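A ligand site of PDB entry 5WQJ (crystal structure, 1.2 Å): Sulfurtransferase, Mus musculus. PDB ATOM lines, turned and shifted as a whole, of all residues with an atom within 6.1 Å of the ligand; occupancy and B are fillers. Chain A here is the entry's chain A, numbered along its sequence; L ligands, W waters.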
ATOM      1  N   TRP A  36     -15.118 -22.852  22.072  1.00  0.00           N
ATOM      2  CA  TRP A  36     -14.974 -22.654  23.528  1.00  0.00           C
ATOM      3  C   TRP A  36     -16.372 -22.698  24.104  1.00  0.00           C
ATOM      4  O   TRP A  36     -17.285 -22.138  23.514  1.00  0.00           O
ATOM      5  CB  TRP A  36     -14.269 -21.308  23.873  1.00  0.00           C
ATOM      6  CG  TRP A  36     -13.899 -21.130  25.335  1.00  0.00           C
ATOM      7  CD1 TRP A  36     -12.702 -21.383  25.879  1.00  0.00           C
ATOM      8  CD2 TRP A  36     -14.765 -20.769  26.413  1.00  0.00           C
ATOM      9  NE1 TRP A  36     -12.727 -21.166  27.230  1.00  0.00           N
ATOM     10  CE2 TRP A  36     -13.972 -20.740  27.572  1.00  0.00           C
ATOM     11  CE3 TRP A  36     -16.084 -20.367  26.499  1.00  0.00           C
ATOM     12  CZ2 TRP A  36     -14.480 -20.425  28.823  1.00  0.00           C
ATOM     13  CZ3 TRP A  36     -16.575 -19.985  27.761  1.00  0.00           C
ATOM     14  CH2 TRP A  36     -15.760 -20.059  28.882  1.00  0.00           C
ATOM     15  N   LEU A  38     -18.898 -22.764  27.783  1.00  0.00           N
ATOM     16  CA  LEU A  38     -19.033 -22.593  29.238  1.00  0.00           C
ATOM     17  C   LEU A  38     -19.041 -23.962  29.932  1.00  0.00           C
ATOM     18  O   LEU A  38     -19.544 -24.969  29.360  1.00  0.00           O
ATOM     19  CB  LEU A  38     -20.299 -21.846  29.573  1.00  0.00           C
ATOM     20  CG  LEU A  38     -20.320 -20.367  29.178  1.00  0.00           C
ATOM     21  CD1 LEU A  38     -21.752 -19.882  29.128  1.00  0.00           C
ATOM     22  CD2 LEU A  38     -19.459 -19.508  30.102  1.00  0.00           C
ATOM     23  N   PRO A  39     -18.439 -24.046  31.128  1.00  0.00           N
ATOM     24  CA  PRO A  39     -18.355 -25.350  31.795  1.00  0.00           C
ATOM     25  C   PRO A  39     -19.624 -26.188  31.864  1.00  0.00           C
ATOM     26  O   PRO A  39     -19.571 -27.402  31.686  1.00  0.00           O
ATOM     27  CB  PRO A  39     -17.904 -24.982  33.180  1.00  0.00           C
ATOM     28  CG  PRO A  39     -17.206 -23.699  33.067  1.00  0.00           C
ATOM     29  CD  PRO A  39     -17.825 -22.976  31.909  1.00  0.00           C
ATOM     30  N   ILE A  62      -8.986 -19.860  22.877  1.00  0.00           N
ATOM     31  CA  ILE A  62      -9.149 -18.483  23.278  1.00  0.00           C
ATOM     32  C   ILE A  62      -8.582 -18.235  24.654  1.00  0.00           C
ATOM     33  O   ILE A  62      -8.249 -17.078  24.993  1.00  0.00           O
ATOM     34  CB  ILE A  62     -10.604 -17.911  23.066  1.00  0.00           C
ATOM     35  CG1 ILE A  62     -11.592 -18.542  24.010  1.00  0.00           C
ATOM     36  CG2 ILE A  62     -11.106 -18.151  21.643  1.00  0.00           C
ATOM     37  CD1 ILE A  62     -12.951 -17.885  23.935  1.00  0.00           C
ATOM     38  N   ASP A  63      -8.384 -19.271  25.458  1.00  0.00           N
ATOM     39  CA  ASP A  63      -7.673 -19.054  26.747  1.00  0.00           C
ATOM     40  C   ASP A  63      -6.173 -18.829  26.525  1.00  0.00           C
ATOM     41  O   ASP A  63      -5.521 -18.361  27.483  1.00  0.00           O
ATOM     42  CB  ASP A  63      -7.946 -20.244  27.674  1.00  0.00           C
ATOM     43  CG  ASP A  63      -9.361 -20.311  28.121  1.00  0.00           C
ATOM     44  OD1 ASP A  63      -9.992 -19.223  28.324  1.00  0.00           O
ATOM     45  OD2 ASP A  63      -9.890 -21.457  28.309  1.00  0.00           O
ATOM     46  N   ASP A  73     -13.239 -11.615  32.602  1.00  0.00           N
ATOM     47  CA  ASP A  73     -13.222 -12.783  31.750  1.00  0.00           C
ATOM     48  C   ASP A  73     -12.944 -12.376  30.309  1.00  0.00           C
ATOM     49  O   ASP A  73     -13.377 -11.342  29.761  1.00  0.00           O
ATOM     50  CB  ASP A  73     -14.548 -13.561  31.888  1.00  0.00           C
ATOM     51  CG  ASP A  73     -14.730 -14.254  33.218  1.00  0.00           C
ATOM     52  OD1 ASP A  73     -13.703 -14.574  33.863  1.00  0.00           O
ATOM     53  OD2 ASP A  73     -15.896 -14.476  33.616  1.00  0.00           O
ATOM     54  N   HIS A  74     -12.272 -13.306  29.627  1.00  0.00           N
ATOM     55  CA  HIS A  74     -11.955 -13.209  28.198  1.00  0.00           C
ATOM     56  C   HIS A  74     -11.531 -11.806  27.762  1.00  0.00           C
ATOM     57  O   HIS A  74     -12.081 -11.213  26.847  1.00  0.00           O
ATOM     58  CB  HIS A  74     -13.130 -13.750  27.366  1.00  0.00           C
ATOM     59  CG  HIS A  74     -13.379 -15.190  27.554  1.00  0.00           C
ATOM     60  ND1 HIS A  74     -12.414 -16.130  27.230  1.00  0.00           N
ATOM     61  CD2 HIS A  74     -14.384 -15.830  28.168  1.00  0.00           C
ATOM     62  CE1 HIS A  74     -12.895 -17.319  27.560  1.00  0.00           C
ATOM     63  NE2 HIS A  74     -14.092 -17.174  28.101  1.00  0.00           N
ATOM     64  N   TYR A 108     -20.504 -19.198  17.514  1.00  0.00           N
ATOM     65  CA  TYR A 108     -20.648 -18.915  18.954  1.00  0.00           C
ATOM     66  C   TYR A 108     -19.471 -18.125  19.482  1.00  0.00           C
ATOM     67  O   TYR A 108     -19.594 -16.931  19.751  1.00  0.00           O
ATOM     68  CB  TYR A 108     -20.830 -20.217  19.752  1.00  0.00           C
ATOM     69  CG  TYR A 108     -21.036 -20.082  21.242  1.00  0.00           C
ATOM     70  CD1 TYR A 108     -22.110 -19.422  21.719  1.00  0.00           C
ATOM     71  CD2 TYR A 108     -20.144 -20.655  22.138  1.00  0.00           C
ATOM     72  CE1 TYR A 108     -22.367 -19.368  23.084  1.00  0.00           C
ATOM     73  CE2 TYR A 108     -20.341 -20.594  23.509  1.00  0.00           C
ATOM     74  CZ  TYR A 108     -21.478 -19.981  23.971  1.00  0.00           C
ATOM     75  OH  TYR A 108     -21.678 -19.980  25.344  1.00  0.00           O
ATOM     76  N   SER A 109     -18.334 -18.785  19.576  1.00  0.00           N
ATOM     77  CA  SER A 109     -17.070 -18.139  19.946  1.00  0.00           C
ATOM     78  C   SER A 109     -16.186 -17.709  18.772  1.00  0.00           C
ATOM     79  O   SER A 109     -15.346 -16.856  18.983  1.00  0.00           O
ATOM     80  CB  SER A 109     -16.318 -19.073  20.879  1.00  0.00           C
ATOM     81  OG  SER A 109     -16.141 -20.338  20.244  1.00  0.00           O
ATOM     82  N   ARG A 184     -26.405 -11.045  25.089  1.00  0.00           N
ATOM     83  CA  ARG A 184     -26.798 -12.170  25.960  1.00  0.00           C
ATOM     84  C   ARG A 184     -28.253 -12.645  25.709  1.00  0.00           C
ATOM     85  O   ARG A 184     -29.098 -11.895  25.250  1.00  0.00           O
ATOM     86  CB  ARG A 184     -26.644 -11.822  27.442  1.00  0.00           C
ATOM     87  CG  ARG A 184     -25.216 -11.805  27.954  1.00  0.00           C
ATOM     88  CD  ARG A 184     -25.088 -11.283  29.379  1.00  0.00           C
ATOM     89  NE  ARG A 184     -25.612  -9.921  29.465  1.00  0.00           N
ATOM     90  CZ  ARG A 184     -26.268  -9.416  30.502  1.00  0.00           C
ATOM     91  NH1 ARG A 184     -26.478 -10.106  31.636  1.00  0.00           N
ATOM     92  NH2 ARG A 184     -26.709  -8.194  30.417  1.00  0.00           N
ATOM     93  N   ARG A 188     -31.045 -13.614  30.774  1.00  0.00           N
ATOM     94  CA  ARG A 188     -29.894 -13.005  31.455  1.00  0.00           C
ATOM     95  C   ARG A 188     -29.993 -11.480  31.434  1.00  0.00           C
ATOM     96  O   ARG A 188     -29.791 -10.831  32.469  1.00  0.00           O
ATOM     97  CB  ARG A 188     -28.573 -13.501  30.787  1.00  0.00           C
ATOM     98  CG  ARG A 188     -28.261 -14.972  31.129  1.00  0.00           C
ATOM     99  CD  ARG A 188     -27.118 -15.554  30.356  1.00  0.00           C
ATOM    100  NE  ARG A 188     -25.884 -14.868  30.677  1.00  0.00           N
ATOM    101  CZ  ARG A 188     -24.775 -15.074  29.995  1.00  0.00           C
ATOM    102  NH1 ARG A 188     -24.752 -15.939  29.018  1.00  0.00           N
ATOM    103  NH2 ARG A 188     -23.687 -14.436  30.332  1.00  0.00           N
ATOM    104  N   GLU A 195     -26.365 -15.886  35.604  1.00  0.00           N
ATOM    105  CA  GLU A 195     -25.077 -15.714  34.977  1.00  0.00           C
ATOM    106  C   GLU A 195     -24.162 -16.882  35.322  1.00  0.00           C
ATOM    107  O   GLU A 195     -24.093 -17.360  36.480  1.00  0.00           O
ATOM    108  CB  GLU A 195     -24.441 -14.407  35.453  1.00  0.00           C
ATOM    109  CG  GLU A 195     -25.102 -13.194  34.856  1.00  0.00           C
ATOM    110  CD  GLU A 195     -24.817 -13.067  33.368  1.00  0.00           C
ATOM    111  OE1 GLU A 195     -23.664 -13.366  32.924  1.00  0.00           O
ATOM    112  OE2 GLU A 195     -25.766 -12.718  32.601  1.00  0.00           O
ATOM    113  N   PRO A 196     -23.414 -17.372  34.300  1.00  0.00           N
ATOM    114  CA  PRO A 196     -22.667 -18.594  34.546  1.00  0.00           C
ATOM    115  C   PRO A 196     -21.551 -18.427  35.585  1.00  0.00           C
ATOM    116  O   PRO A 196     -21.161 -19.367  36.296  1.00  0.00           O
ATOM    117  CB  PRO A 196     -22.150 -18.985  33.146  1.00  0.00           C
ATOM    118  CG  PRO A 196     -22.350 -17.803  32.272  1.00  0.00           C
ATOM    119  CD  PRO A 196     -23.408 -16.946  32.890  1.00  0.00           C
ATOM    120  N   ARG A 197     -21.049 -17.189  35.736  1.00  0.00           N
ATOM    121  CA  ARG A 197     -19.973 -16.904  36.633  1.00  0.00           C
ATOM    122  C   ARG A 197     -20.535 -16.810  38.073  1.00  0.00           C
ATOM    123  O   ARG A 197     -21.483 -16.107  38.336  1.00  0.00           O
ATOM    124  CB  ARG A 197     -19.334 -15.633  36.096  1.00  0.00           C
ATOM    125  CG  ARG A 197     -17.997 -15.179  36.671  1.00  0.00           C
ATOM    126  CD  ARG A 197     -16.984 -16.281  36.822  1.00  0.00           C
ATOM    127  NE  ARG A 197     -15.964 -16.309  35.817  1.00  0.00           N
ATOM    128  CZ  ARG A 197     -15.005 -17.226  35.810  1.00  0.00           C
ATOM    129  NH1 ARG A 197     -14.066 -17.175  34.908  1.00  0.00           N
ATOM    130  NH2 ARG A 197     -14.984 -18.216  36.700  1.00  0.00           N
ATOM    131  N   ASP A 198     -19.968 -17.571  38.988  1.00  0.00           N
ATOM    132  CA  ASP A 198     -20.356 -17.431  40.380  1.00  0.00           C
ATOM    133  C   ASP A 198     -19.960 -16.043  40.901  1.00  0.00           C
ATOM    134  O   ASP A 198     -18.916 -15.498  40.548  1.00  0.00           O
ATOM    135  CB  ASP A 198     -19.730 -18.518  41.230  1.00  0.00           C
ATOM    136  CG  ASP A 198     -20.211 -18.443  42.650  1.00  0.00           C
ATOM    137  OD1 ASP A 198     -19.351 -18.352  43.540  1.00  0.00           O
ATOM    138  OD2 ASP A 198     -21.438 -18.400  42.857  1.00  0.00           O
ATOM    139  N   PHE A 213     -27.606 -12.996  20.632  1.00  0.00           N
ATOM    140  CA  PHE A 213     -26.773 -13.265  19.449  1.00  0.00           C
ATOM    141  C   PHE A 213     -27.485 -14.231  18.487  1.00  0.00           C
ATOM    142  O   PHE A 213     -27.207 -14.208  17.286  1.00  0.00           O
ATOM    143  CB  PHE A 213     -25.358 -13.736  19.817  1.00  0.00           C
ATOM    144  CG  PHE A 213     -25.300 -15.146  20.392  1.00  0.00           C
ATOM    145  CD1 PHE A 213     -25.530 -15.401  21.749  1.00  0.00           C
ATOM    146  CD2 PHE A 213     -25.108 -16.254  19.549  1.00  0.00           C
ATOM    147  CE1 PHE A 213     -25.446 -16.677  22.242  1.00  0.00           C
ATOM    148  CE2 PHE A 213     -25.104 -17.535  20.056  1.00  0.00           C
ATOM    149  CZ  PHE A 213     -25.304 -17.748  21.408  1.00  0.00           C
ATOM    150  N   CSS A 248     -21.771  -8.194  26.121  1.00  0.00           N
ATOM    151  CA  CSS A 248     -22.421  -9.475  26.402  1.00  0.00           C
ATOM    152  CB  CSS A 248     -22.098 -10.527  25.301  1.00  0.00           C
ATOM    153  SG  CSS A 248     -20.394 -11.003  25.176  1.00  0.00           S
ATOM    154  SD  CSS A 248     -20.249 -13.095  25.894  1.00  0.00           S
ATOM    155  C   CSS A 248     -21.976  -9.907  27.809  1.00  0.00           C
ATOM    156  O   CSS A 248     -21.807  -9.044  28.663  1.00  0.00           O
ATOM    157  N   GLY A 249     -21.765 -11.179  28.025  1.00  0.00           N
ATOM    158  CA  GLY A 249     -21.228 -11.640  29.307  1.00  0.00           C
ATOM    159  C   GLY A 249     -19.785 -11.321  29.570  1.00  0.00           C
ATOM    160  O   GLY A 249     -19.470 -10.744  30.606  1.00  0.00           O
ATOM    161  N   SER A 250     -18.944 -11.615  28.568  1.00  0.00           N
ATOM    162  CA  SER A 250     -17.500 -11.403  28.706  1.00  0.00           C
ATOM    163  C   SER A 250     -16.790 -10.869  27.472  1.00  0.00           C
ATOM    164  O   SER A 250     -15.573 -10.920  27.409  1.00  0.00           O
ATOM    165  CB  SER A 250     -16.756 -12.635  29.169  1.00  0.00           C
ATOM    166  OG  SER A 250     -16.908 -13.691  28.280  1.00  0.00           O
ATOM    167  N   GLY A 251     -17.562 -10.439  26.477  1.00  0.00           N
ATOM    168  CA  GLY A 251     -17.025  -9.852  25.321  1.00  0.00           C
ATOM    169  C   GLY A 251     -16.934 -10.800  24.146  1.00  0.00           C
ATOM    170  O   GLY A 251     -16.334 -10.443  23.113  1.00  0.00           O
ATOM    171  N   VAL A 252     -17.401 -12.032  24.273  1.00  0.00           N
ATOM    172  CA  VAL A 252     -17.298 -13.057  23.219  1.00  0.00           C
ATOM    173  C   VAL A 252     -18.484 -12.971  22.231  1.00  0.00           C
ATOM    174  O   VAL A 252     -18.289 -12.618  21.073  1.00  0.00           O
ATOM    175  CB  VAL A 252     -17.161 -14.456  23.855  1.00  0.00           C
ATOM    176  CG1 VAL A 252     -17.099 -15.480  22.783  1.00  0.00           C
ATOM    177  CG2 VAL A 252     -15.898 -14.525  24.682  1.00  0.00           C
ATOM    178  N   THR A 253     -19.699 -13.229  22.703  1.00  0.00           N
ATOM    179  CA  THR A 253     -20.834 -13.213  21.804  1.00  0.00           C
ATOM    180  C   THR A 253     -21.190 -11.800  21.332  1.00  0.00           C
ATOM    181  O   THR A 253     -21.924 -11.666  20.376  1.00  0.00           O
ATOM    182  CB  THR A 253     -22.064 -13.944  22.386  1.00  0.00           C
ATOM    183  OG1 THR A 253     -22.525 -13.286  23.538  1.00  0.00           O
ATOM    184  CG2 THR A 253     -21.765 -15.387  22.648  1.00  0.00           C
ATOM    185  N   VAL A 277     -19.595  -9.140  33.166  1.00  0.00           N
ATOM    186  CA  VAL A 277     -18.786  -9.533  34.325  1.00  0.00           C
ATOM    187  C   VAL A 277     -18.081  -8.352  34.978  1.00  0.00           C
ATOM    188  O   VAL A 277     -18.270  -8.133  36.182  1.00  0.00           O
ATOM    189  CB  VAL A 277     -17.781 -10.660  33.967  1.00  0.00           C
ATOM    190  CG1 VAL A 277     -16.812 -10.907  35.078  1.00  0.00           C
ATOM    191  CG2 VAL A 277     -18.490 -11.940  33.594  1.00  0.00           C
HETATM  192  O1  LIG L   1     -22.591 -15.985  27.202  1.00  0.00           O
HETATM  193  C1  LIG L   1     -21.472 -15.912  27.688  1.00  0.00           C
HETATM  194  C2  LIG L   1     -20.336 -16.444  26.914  1.00  0.00           C
HETATM  195  C3  LIG L   1     -20.394 -17.052  25.644  1.00  0.00           C
HETATM  196  C4  LIG L   1     -19.243 -17.523  25.030  1.00  0.00           C
HETATM  197  C5  LIG L   1     -18.050 -17.432  25.696  1.00  0.00           C
HETATM  198  C6  LIG L   1     -17.915 -16.829  26.912  1.00  0.00           C
HETATM  199  C7  LIG L   1     -19.025 -16.370  27.563  1.00  0.00           C
HETATM  200  N1  LIG L   1     -21.200 -15.382  28.862  1.00  0.00           N
HETATM  201  C8  LIG L   1     -19.984 -15.369  29.411  1.00  0.00           C
HETATM  202  N2  LIG L   1     -18.877 -15.791  28.793  1.00  0.00           N
HETATM  203  S1  LIG L   1     -19.847 -14.531  30.925  1.00  0.00           S
HETATM  204  C9  LIG L   1     -18.267 -15.053  31.483  1.00  0.00           C
HETATM  205  C10 LIG L   1     -18.285 -16.388  32.203  1.00  0.00           C
HETATM  206  O2  LIG L   1     -19.215 -16.775  32.893  1.00  0.00           O
HETATM  207  N3  LIG L   1     -17.192 -17.126  32.064  1.00  0.00           N
HETATM  208  C11 LIG L   1     -17.066 -18.271  32.765  1.00  0.00           C
HETATM  209  S2  LIG L   1     -18.163 -19.046  33.841  1.00  0.00           S
HETATM  210  C12 LIG L   1     -17.007 -20.301  34.210  1.00  0.00           C
HETATM  211  C13 LIG L   1     -15.784 -20.152  33.574  1.00  0.00           C
HETATM  212  C14 LIG L   1     -15.785 -19.006  32.776  1.00  0.00           C
HETATM  213  C15 LIG L   1     -14.644 -18.523  31.972  1.00  0.00           C
HETATM  214  O3  LIG L   1     -14.704 -17.465  31.366  1.00  0.00           O
HETATM  215  N4  LIG L   1     -13.495 -19.203  32.012  1.00  0.00           N
HETATM  216  O   HOH W   1     -21.234 -14.723  34.123  1.00  0.00           O
HETATM  217  O   HOH W   2     -24.112 -14.478  25.504  1.00  0.00           O
HETATM  218  O   HOH W   3     -10.995 -18.512  30.689  1.00  0.00           O
HETATM  219  O   HOH W   4     -12.184 -15.908  30.858  1.00  0.00           O
HETATM  220  O   HOH W   5     -23.598 -18.363  26.145  1.00  0.00           O
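The backbone NH (N) of Arg 197 sits close to an oxygen (O2) of the ligand. NH1 of Arg 188 is in hydrogen-bond range of O1 of the ligand (2.8 Å). A nitrogen (N3) of the ligand sits close to the side-chain carboxylate (OD2) of Asp 73 (3.3 Å). OG of Ser 250 is in hydrogen-bond range of N2 of the ligand, 2.9 Å away. A ring nitrogen (NE2) of His 74 is in hydrogen-bond range of an oxygen (O3) of the ligand (3.3 Å).
Water W2 bridges an oxygen (O1) of the ligand (2.7 Å) and the side-chain hydroxyl of Thr 253 (2.8 Å). Water W5 bridges OH of Tyr 108 (2.6 Å) and O1 of the ligand (2.8 Å). Water W3 lies within hydrogen-bond range of the side-chain carboxylate of Asp 63 (2.7 Å) and a nitrogen (N4) of the ligand (2.9 Å). Water W4 bridges the backbone NH (N) of His 74 (2.9 Å) and an oxygen (O3) of the ligand (3.0 Å). Water W1 lies within hydrogen-bond range of N of Arg 197 (3.0 Å), OE1 of Glu 195 (3.0 Å) and O2 of the ligand (3.1 Å).
The side-chain carboxylate (OE1) of Glu 195 is in salt-bridge range of the guanidinium group (NH2) of Arg 188 (2.8 Å). The backbone NH (N) of Ser 250 is in hydrogen-bond range of SD of CSS 248, 3.3 Å away. The backbone carbonyl oxygen of Arg 188 is in hydrogen-bond range of the guanidinium group of Arg 184, at 3.5 Å. OD2 of Asp 63 sits at hydrogen-bond distance from NE1 of Trp 36 (3.0 Å). The side-chain hydroxyl of Ser 109 sits at hydrogen-bond distance from the backbone NH of Trp 36. N of Val 277 lies within hydrogen-bond range of O of Gly 249 (3.0 Å). SG of CSS 248 lies within hydrogen-bond range of the backbone NH (N) of Gly 251 (3.2 Å). SG of CSS 248 lies within hydrogen-bond range of N of Val 252 (3.3 Å).
Merely in contact with the ligand: Trp 36, Leu 38, Pro 39, Tyr 108, Pro 196, CSS 248, Gly 249, Val 252, Thr 253 and Val 277. Hydrophobic or aromatic side chains within 4 Å of the ligand: Trp 36, Leu 38, Pro 39, His 74, Tyr 108, Pro 196, Val 252 and Val 277. The nearest printed residue that does not touch the ligand is Glu 195 (4.5 Å).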
